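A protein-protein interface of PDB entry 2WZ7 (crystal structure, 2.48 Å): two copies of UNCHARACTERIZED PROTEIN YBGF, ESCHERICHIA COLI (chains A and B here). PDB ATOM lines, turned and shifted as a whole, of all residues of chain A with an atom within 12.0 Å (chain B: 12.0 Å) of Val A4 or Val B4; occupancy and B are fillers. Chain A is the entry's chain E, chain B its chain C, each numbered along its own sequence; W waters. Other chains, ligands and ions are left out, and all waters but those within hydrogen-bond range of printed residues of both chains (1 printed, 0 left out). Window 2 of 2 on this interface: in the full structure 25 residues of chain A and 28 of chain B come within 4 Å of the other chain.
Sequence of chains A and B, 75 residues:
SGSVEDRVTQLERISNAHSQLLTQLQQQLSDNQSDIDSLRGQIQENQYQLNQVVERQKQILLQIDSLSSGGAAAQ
The side-chain carboxylate of Glu B12 is in salt-bridge range of the guanidinium group of Arg A7, 2.7 Å away.
The side-chain hydroxyl of Thr B9 is in hydrogen-bond range of the backbone carbonyl oxygen of Glu B5 (2.8 Å).
Among the printed residues, pairs that only touch across the chains: Val A4 with Val B4 (3.7 Å), Arg A7 with Glu B5 (3.9 Å), Arg A7 with Val B8 (3.6 Å), Arg A7 with Thr B9 (3.6 Å), Val A8 with Val B8 (3.9 Å), Leu A11 with Val B8 (3.9 Å), Leu A11 with Leu B11 (3.7 Å) and Leu A11 with Glu B12 (3.8 Å).
Printed residues of chain B within 4 Å of Val A4: Val B4 (3.7 Å).
Of chain A, only Val A4 comes within 4 Å of Val B4.
Gly A2 touches none of the printed residues of chain B.
No residue of chain B comes within 4 Å of Glu A5.
No residue of chain B comes within 4 Å of Asp A6.
Of chain B, only Glu B5, Val B8, Thr B9 and Glu B12 come within 4 Å of Arg A7.
Val A8 touches just one residue of chain B: Val B8 (3.9 Å).
No residue of chain A comes within 4 Å of Ser B3.
No residue of chain A comes within 4 Å of Asp B6.
Val B8 touches just these residues of chain A: Arg A7 (3.6 Å), Val A8 (3.9 Å) and Leu A11 (3.9 Å).
Printed residues of chain B within 4 Å of Leu A11: Val B8, Leu B11 and Glu B12.
Printed residues of chain A within 4 Å of Glu B12: Arg A7 (2.7 Å) and Leu A11 (3.8 Å).
Of the printed residues of chain A, Leu B11 touches Leu A11 (3.7 Å).
Printed residues of chain A within 4 Å of Thr B9: Arg A7.
Of the printed residues of chain A, Glu B5 touches Arg A7.
Glu A12 touches none of the printed residues of chain B.
Gln A10 touches none of the printed residues of chain B.
The nearest printed residue of chain B that does not touch Val A4 is Glu B5 (4.02 Å).
The nearest residue of chain A that does not touch Val B4 is Arg A7 (5.9 Å).
Hydrophobic or aromatic side chains of chain B within 4 Å of the printed part of chain A: Val B4, Val B8 and Leu B11.
Along chain B the printed residues that touch a printed residue of chain A span positions 4 to 12.
Of the 12 printed residues of chain A, 4 touch a printed residue of chain B.
Along chain A the printed residues that touch a printed residue of chain B span positions 4 to 11.
Val B4 touches its own counterpart, Val A4.
Arg A7 touches Glu B12, but with the chains exchanged Glu A12 does not touch Arg B7 (11.2 Å).
Leu A11 touches Val B8, but with the chains exchanged Val A8 does not touch Leu B11 (6.4 Å).
Leu A11 touches Glu B12, but with the chains exchanged Glu A12 does not touch Leu B11 (7.8 Å).
Positions printed for both chains: 3, 4, 5, 6, 7, 8, 9, 10, 11, 12 and 13.
Water W1 bridges OE2 of Glu B12 (2.6 Å) and O of Arg A7 (2.7 Å).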
ATOM      1  N   GLY A   2      -1.428  33.083  -2.341  1.00  0.00           N
ATOM      2  CA  GLY A   2      -2.309  33.588  -1.252  1.00  0.00           C
ATOM      3  C   GLY A   2      -3.706  32.985  -1.269  1.00  0.00           C
ATOM      4  O   GLY A   2      -3.871  31.771  -1.474  1.00  0.00           O
ATOM      5  N   SER A   3      -4.706  33.842  -1.040  1.00  0.00           N
ATOM      6  CA  SER A   3      -6.089  33.417  -0.857  1.00  0.00           C
ATOM      7  C   SER A   3      -6.678  32.803  -2.123  1.00  0.00           C
ATOM      8  O   SER A   3      -6.329  33.197  -3.249  1.00  0.00           O
ATOM      9  CB  SER A   3      -6.946  34.606  -0.415  1.00  0.00           C
ATOM     10  OG  SER A   3      -7.006  35.608  -1.421  1.00  0.00           O
ATOM     11  N   VAL A   4      -7.577  31.841  -1.942  1.00  0.00           N
ATOM     12  CA  VAL A   4      -8.333  31.295  -3.056  1.00  0.00           C
ATOM     13  C   VAL A   4      -8.906  32.421  -3.952  1.00  0.00           C
ATOM     14  O   VAL A   4      -8.889  32.290  -5.179  1.00  0.00           O
ATOM     15  CB  VAL A   4      -9.410  30.298  -2.587  1.00  0.00           C
ATOM     16  CG1 VAL A   4     -10.339  29.905  -3.732  1.00  0.00           C
ATOM     17  CG2 VAL A   4      -8.746  29.045  -2.013  1.00  0.00           C
ATOM     18  N   GLU A   5      -9.372  33.517  -3.345  1.00  0.00           N
ATOM     19  CA  GLU A   5      -9.771  34.719  -4.073  1.00  0.00           C
ATOM     20  C   GLU A   5      -8.691  35.205  -5.051  1.00  0.00           C
ATOM     21  O   GLU A   5      -8.972  35.467  -6.224  1.00  0.00           O
ATOM     22  CB  GLU A   5     -10.049  35.858  -3.093  1.00  0.00           C
ATOM     23  CG  GLU A   5     -11.512  36.159  -2.790  1.00  0.00           C
ATOM     24  CD  GLU A   5     -11.673  37.512  -2.078  1.00  0.00           C
ATOM     25  OE1 GLU A   5     -12.507  38.342  -2.535  1.00  0.00           O
ATOM     26  OE2 GLU A   5     -10.945  37.756  -1.073  1.00  0.00           O
ATOM     27  N   ASP A   6      -7.465  35.350  -4.552  1.00  0.00           N
ATOM     28  CA  ASP A   6      -6.368  35.859  -5.371  1.00  0.00           C
ATOM     29  C   ASP A   6      -6.049  34.891  -6.501  1.00  0.00           C
ATOM     30  O   ASP A   6      -5.952  35.303  -7.650  1.00  0.00           O
ATOM     31  CB  ASP A   6      -5.125  36.162  -4.525  1.00  0.00           C
ATOM     32  CG  ASP A   6      -5.323  37.359  -3.609  1.00  0.00           C
ATOM     33  OD1 ASP A   6      -6.386  38.022  -3.725  1.00  0.00           O
ATOM     34  OD2 ASP A   6      -4.427  37.637  -2.770  1.00  0.00           O
ATOM     35  N   ARG A   7      -5.932  33.609  -6.175  1.00  0.00           N
ATOM     36  CA  ARG A   7      -5.634  32.594  -7.161  1.00  0.00           C
ATOM     37  C   ARG A   7      -6.691  32.519  -8.290  1.00  0.00           C
ATOM     38  O   ARG A   7      -6.369  32.187  -9.438  1.00  0.00           O
ATOM     39  CB  ARG A   7      -5.413  31.240  -6.486  1.00  0.00           C
ATOM     40  CG  ARG A   7      -4.242  31.184  -5.506  1.00  0.00           C
ATOM     41  CD  ARG A   7      -3.681  29.768  -5.391  1.00  0.00           C
ATOM     42  NE  ARG A   7      -4.452  28.915  -4.490  1.00  0.00           N
ATOM     43  CZ  ARG A   7      -4.689  27.611  -4.651  1.00  0.00           C
ATOM     44  NH1 ARG A   7      -4.245  26.942  -5.705  1.00  0.00           N
ATOM     45  NH2 ARG A   7      -5.398  26.971  -3.731  1.00  0.00           N
ATOM     46  N   VAL A   8      -7.935  32.879  -7.975  1.00  0.00           N
ATOM     47  CA  VAL A   8      -9.033  32.818  -8.942  1.00  0.00           C
ATOM     48  C   VAL A   8      -8.979  34.017  -9.866  1.00  0.00           C
ATOM     49  O   VAL A   8      -9.245  33.899 -11.075  1.00  0.00           O
ATOM     50  CB  VAL A   8     -10.399  32.714  -8.259  1.00  0.00           C
ATOM     51  CG1 VAL A   8     -11.513  33.160  -9.186  1.00  0.00           C
ATOM     52  CG2 VAL A   8     -10.651  31.280  -7.826  1.00  0.00           C
ATOM     53  N   THR A   9      -8.622  35.164  -9.295  1.00  0.00           N
ATOM     54  CA  THR A   9      -8.509  36.405 -10.051  1.00  0.00           C
ATOM     55  C   THR A   9      -7.371  36.231 -11.058  1.00  0.00           C
ATOM     56  O   THR A   9      -7.546  36.515 -12.239  1.00  0.00           O
ATOM     57  CB  THR A   9      -8.293  37.619  -9.097  1.00  0.00           C
ATOM     58  OG1 THR A   9      -9.511  37.864  -8.367  1.00  0.00           O
ATOM     59  CG2 THR A   9      -7.877  38.906  -9.858  1.00  0.00           C
ATOM     60  N   GLN A  10      -6.235  35.719 -10.578  1.00  0.00           N
ATOM     61  CA  GLN A  10      -5.085  35.396 -11.414  1.00  0.00           C
ATOM     62  C   GLN A  10      -5.471  34.458 -12.580  1.00  0.00           C
ATOM     63  O   GLN A  10      -5.301  34.832 -13.750  1.00  0.00           O
ATOM     64  CB  GLN A  10      -3.933  34.830 -10.562  1.00  0.00           C
ATOM     65  CG  GLN A  10      -2.567  34.644 -11.282  1.00  0.00           C
ATOM     66  CD  GLN A  10      -1.905  35.953 -11.819  1.00  0.00           C
ATOM     67  OE1 GLN A  10      -2.364  37.077 -11.565  1.00  0.00           O
ATOM     68  NE2 GLN A  10      -0.802  35.783 -12.557  1.00  0.00           N
ATOM     69  N   LEU A  11      -6.012  33.280 -12.260  1.00  0.00           N
ATOM     70  CA  LEU A  11      -6.556  32.353 -13.259  1.00  0.00           C
ATOM     71  C   LEU A  11      -7.431  33.014 -14.333  1.00  0.00           C
ATOM     72  O   LEU A  11      -7.356  32.643 -15.499  1.00  0.00           O
ATOM     73  CB  LEU A  11      -7.329  31.201 -12.585  1.00  0.00           C
ATOM     74  CG  LEU A  11      -6.491  30.045 -11.998  1.00  0.00           C
ATOM     75  CD1 LEU A  11      -7.226  29.207 -10.943  1.00  0.00           C
ATOM     76  CD2 LEU A  11      -5.926  29.134 -13.117  1.00  0.00           C
ATOM     77  N   GLU A  12      -8.248  33.991 -13.937  1.00  0.00           N
ATOM     78  CA  GLU A  12      -9.118  34.728 -14.865  1.00  0.00           C
ATOM     79  C   GLU A  12      -8.335  35.634 -15.816  1.00  0.00           C
ATOM     80  O   GLU A  12      -8.709  35.820 -16.972  1.00  0.00           O
ATOM     81  CB  GLU A  12     -10.131  35.569 -14.097  1.00  0.00           C
ATOM     82  CG  GLU A  12     -11.278  34.783 -13.505  1.00  0.00           C
ATOM     83  CD  GLU A  12     -12.050  35.543 -12.420  1.00  0.00           C
ATOM     84  OE1 GLU A  12     -11.522  36.543 -11.877  1.00  0.00           O
ATOM     85  OE2 GLU A  12     -13.197  35.123 -12.105  1.00  0.00           O
ATOM     86  N   ARG A  13      -7.252  36.198 -15.311  1.00  0.00           N
ATOM     87  CA  ARG A  13      -6.403  37.101 -16.047  1.00  0.00           C
ATOM     88  C   ARG A  13      -5.540  36.310 -17.052  1.00  0.00           C
ATOM     89  O   ARG A  13      -5.508  36.636 -18.251  1.00  0.00           O
ATOM     90  CB  ARG A  13      -5.593  37.901 -15.026  1.00  0.00           C
ATOM     91  CG  ARG A  13      -4.214  38.414 -15.431  1.00  0.00           C
ATOM     92  CD  ARG A  13      -3.667  39.379 -14.341  1.00  0.00           C
ATOM     93  NE  ARG A  13      -4.442  40.627 -14.285  1.00  0.00           N
ATOM     94  CZ  ARG A  13      -5.465  40.862 -13.459  1.00  0.00           C
ATOM     95  NH1 ARG A  13      -5.860  39.946 -12.576  1.00  0.00           N
ATOM     96  NH2 ARG A  13      -6.096  42.032 -13.522  1.00  0.00           N
ATOM     97  N   SER B   3     -13.060  21.050  -1.916  1.00  0.00           N
ATOM     98  CA  SER B   3     -12.797  20.669  -3.316  1.00  0.00           C
ATOM     99  C   SER B   3     -12.438  21.943  -4.063  1.00  0.00           C
ATOM    100  O   SER B   3     -11.681  21.883  -5.031  1.00  0.00           O
ATOM    101  CB  SER B   3     -13.993  19.959  -3.968  1.00  0.00           C
ATOM    102  OG  SER B   3     -13.563  18.838  -4.725  1.00  0.00           O
ATOM    103  N   VAL B   4     -12.966  23.092  -3.617  1.00  0.00           N
ATOM    104  CA  VAL B   4     -12.631  24.403  -4.237  1.00  0.00           C
ATOM    105  C   VAL B   4     -11.112  24.643  -4.407  1.00  0.00           C
ATOM    106  O   VAL B   4     -10.655  24.951  -5.516  1.00  0.00           O
ATOM    107  CB  VAL B   4     -13.264  25.603  -3.490  1.00  0.00           C
ATOM    108  CG1 VAL B   4     -12.314  26.796  -3.505  1.00  0.00           C
ATOM    109  CG2 VAL B   4     -14.648  25.973  -4.088  1.00  0.00           C
ATOM    110  N   GLU B   5     -10.360  24.492  -3.310  1.00  0.00           N
ATOM    111  CA  GLU B   5      -8.904  24.490  -3.328  1.00  0.00           C
ATOM    112  C   GLU B   5      -8.327  23.524  -4.362  1.00  0.00           C
ATOM    113  O   GLU B   5      -7.314  23.837  -4.996  1.00  0.00           O
ATOM    114  CB  GLU B   5      -8.359  24.095  -1.958  1.00  0.00           C
ATOM    115  CG  GLU B   5      -8.342  25.196  -0.941  1.00  0.00           C
ATOM    116  CD  GLU B   5      -9.505  25.110   0.068  1.00  0.00           C
ATOM    117  OE1 GLU B   5     -10.604  24.560  -0.271  1.00  0.00           O
ATOM    118  OE2 GLU B   5      -9.299  25.609   1.209  1.00  0.00           O
ATOM    119  N   ASP B   6      -8.958  22.349  -4.489  1.00  0.00           N
ATOM    120  CA  ASP B   6      -8.508  21.273  -5.374  1.00  0.00           C
ATOM    121  C   ASP B   6      -8.878  21.538  -6.833  1.00  0.00           C
ATOM    122  O   ASP B   6      -8.085  21.263  -7.743  1.00  0.00           O
ATOM    123  CB  ASP B   6      -9.126  19.927  -4.961  1.00  0.00           C
ATOM    124  CG  ASP B   6      -8.574  19.372  -3.644  1.00  0.00           C
ATOM    125  OD1 ASP B   6      -7.568  19.875  -3.071  1.00  0.00           O
ATOM    126  OD2 ASP B   6      -9.178  18.377  -3.187  1.00  0.00           O
ATOM    127  N   ARG B   7     -10.100  22.017  -7.059  1.00  0.00           N
ATOM    128  CA  ARG B   7     -10.531  22.411  -8.394  1.00  0.00           C
ATOM    129  C   ARG B   7      -9.625  23.550  -8.889  1.00  0.00           C
ATOM    130  O   ARG B   7      -9.113  23.489 -10.002  1.00  0.00           O
ATOM    131  CB  ARG B   7     -11.985  22.835  -8.400  1.00  0.00           C
ATOM    132  CG  ARG B   7     -12.981  21.708  -8.243  1.00  0.00           C
ATOM    133  CD  ARG B   7     -14.298  22.244  -7.694  1.00  0.00           C
ATOM    134  NE  ARG B   7     -15.006  22.978  -8.736  1.00  0.00           N
ATOM    135  CZ  ARG B   7     -16.085  23.736  -8.546  1.00  0.00           C
ATOM    136  NH1 ARG B   7     -16.605  23.878  -7.324  1.00  0.00           N
ATOM    137  NH2 ARG B   7     -16.636  24.362  -9.582  1.00  0.00           N
ATOM    138  N   VAL B   8      -9.384  24.541  -8.030  1.00  0.00           N
ATOM    139  CA  VAL B   8      -8.491  25.650  -8.331  1.00  0.00           C
ATOM    140  C   VAL B   8      -7.072  25.150  -8.654  1.00  0.00           C
ATOM    141  O   VAL B   8      -6.507  25.569  -9.663  1.00  0.00           O
ATOM    142  CB  VAL B   8      -8.515  26.733  -7.200  1.00  0.00           C
ATOM    143  CG1 VAL B   8      -7.340  27.670  -7.295  1.00  0.00           C
ATOM    144  CG2 VAL B   8      -9.764  27.519  -7.292  1.00  0.00           C
ATOM    145  N   THR B   9      -6.507  24.265  -7.819  1.00  0.00           N
ATOM    146  CA  THR B   9      -5.189  23.665  -8.095  1.00  0.00           C
ATOM    147  C   THR B   9      -5.163  22.954  -9.461  1.00  0.00           C
ATOM    148  O   THR B   9      -4.219  23.128 -10.221  1.00  0.00           O
ATOM    149  CB  THR B   9      -4.721  22.687  -6.978  1.00  0.00           C
ATOM    150  OG1 THR B   9      -4.642  23.382  -5.741  1.00  0.00           O
ATOM    151  CG2 THR B   9      -3.336  22.135  -7.271  1.00  0.00           C
ATOM    152  N   GLN B  10      -6.204  22.174  -9.761  1.00  0.00           N
ATOM    153  CA  GLN B  10      -6.359  21.541 -11.071  1.00  0.00           C
ATOM    154  C   GLN B  10      -6.355  22.585 -12.203  1.00  0.00           C
ATOM    155  O   GLN B  10      -5.750  22.376 -13.263  1.00  0.00           O
ATOM    156  CB  GLN B  10      -7.641  20.678 -11.126  1.00  0.00           C
ATOM    157  CG  GLN B  10      -7.764  19.748 -12.353  1.00  0.00           C
ATOM    158  CD  GLN B  10      -6.569  18.755 -12.506  1.00  0.00           C
ATOM    159  OE1 GLN B  10      -5.669  18.679 -11.644  1.00  0.00           O
ATOM    160  NE2 GLN B  10      -6.566  17.999 -13.610  1.00  0.00           N
ATOM    161  N   LEU B  11      -7.019  23.714 -11.952  1.00  0.00           N
ATOM    162  CA  LEU B  11      -7.117  24.788 -12.939  1.00  0.00           C
ATOM    163  C   LEU B  11      -5.764  25.423 -13.208  1.00  0.00           C
ATOM    164  O   LEU B  11      -5.447  25.704 -14.355  1.00  0.00           O
ATOM    165  CB  LEU B  11      -8.136  25.838 -12.501  1.00  0.00           C
ATOM    166  CG  LEU B  11      -9.560  25.701 -13.058  1.00  0.00           C
ATOM    167  CD1 LEU B  11     -10.115  24.285 -12.936  1.00  0.00           C
ATOM    168  CD2 LEU B  11     -10.485  26.704 -12.360  1.00  0.00           C
ATOM    169  N   GLU B  12      -4.970  25.607 -12.156  1.00  0.00           N
ATOM    170  CA  GLU B  12      -3.662  26.246 -12.258  1.00  0.00           C
ATOM    171  C   GLU B  12      -2.669  25.350 -12.973  1.00  0.00           C
ATOM    172  O   GLU B  12      -1.778  25.824 -13.679  1.00  0.00           O
ATOM    173  CB  GLU B  12      -3.110  26.591 -10.879  1.00  0.00           C
ATOM    174  CG  GLU B  12      -3.979  27.490 -10.080  1.00  0.00           C
ATOM    175  CD  GLU B  12      -3.443  27.729  -8.692  1.00  0.00           C
ATOM    176  OE1 GLU B  12      -2.862  26.811  -8.069  1.00  0.00           O
ATOM    177  OE2 GLU B  12      -3.615  28.853  -8.208  1.00  0.00           O
ATOM    178  N   ARG B  13      -2.819  24.050 -12.767  1.00  0.00           N
ATOM    179  CA  ARG B  13      -2.020  23.072 -13.481  1.00  0.00           C
ATOM    180  C   ARG B  13      -2.340  23.059 -14.988  1.00  0.00           C
ATOM    181  O   ARG B  13      -1.411  23.118 -15.812  1.00  0.00           O
ATOM    182  CB  ARG B  13      -2.143  21.685 -12.829  1.00  0.00           C
ATOM    183  CG  ARG B  13      -1.185  21.557 -11.641  1.00  0.00           C
ATOM    184  CD  ARG B  13      -1.328  20.291 -10.813  1.00  0.00           C
ATOM    185  NE  ARG B  13      -0.185  20.167  -9.897  1.00  0.00           N
ATOM    186  CZ  ARG B  13      -0.193  19.485  -8.751  1.00  0.00           C
ATOM    187  NH1 ARG B  13      -1.282  18.850  -8.359  1.00  0.00           N
ATOM    188  NH2 ARG B  13       0.898  19.435  -7.999  1.00  0.00           N
HETATM  189  O   HOH W   1      -4.013  30.888  -9.826  1.00  0.00           O
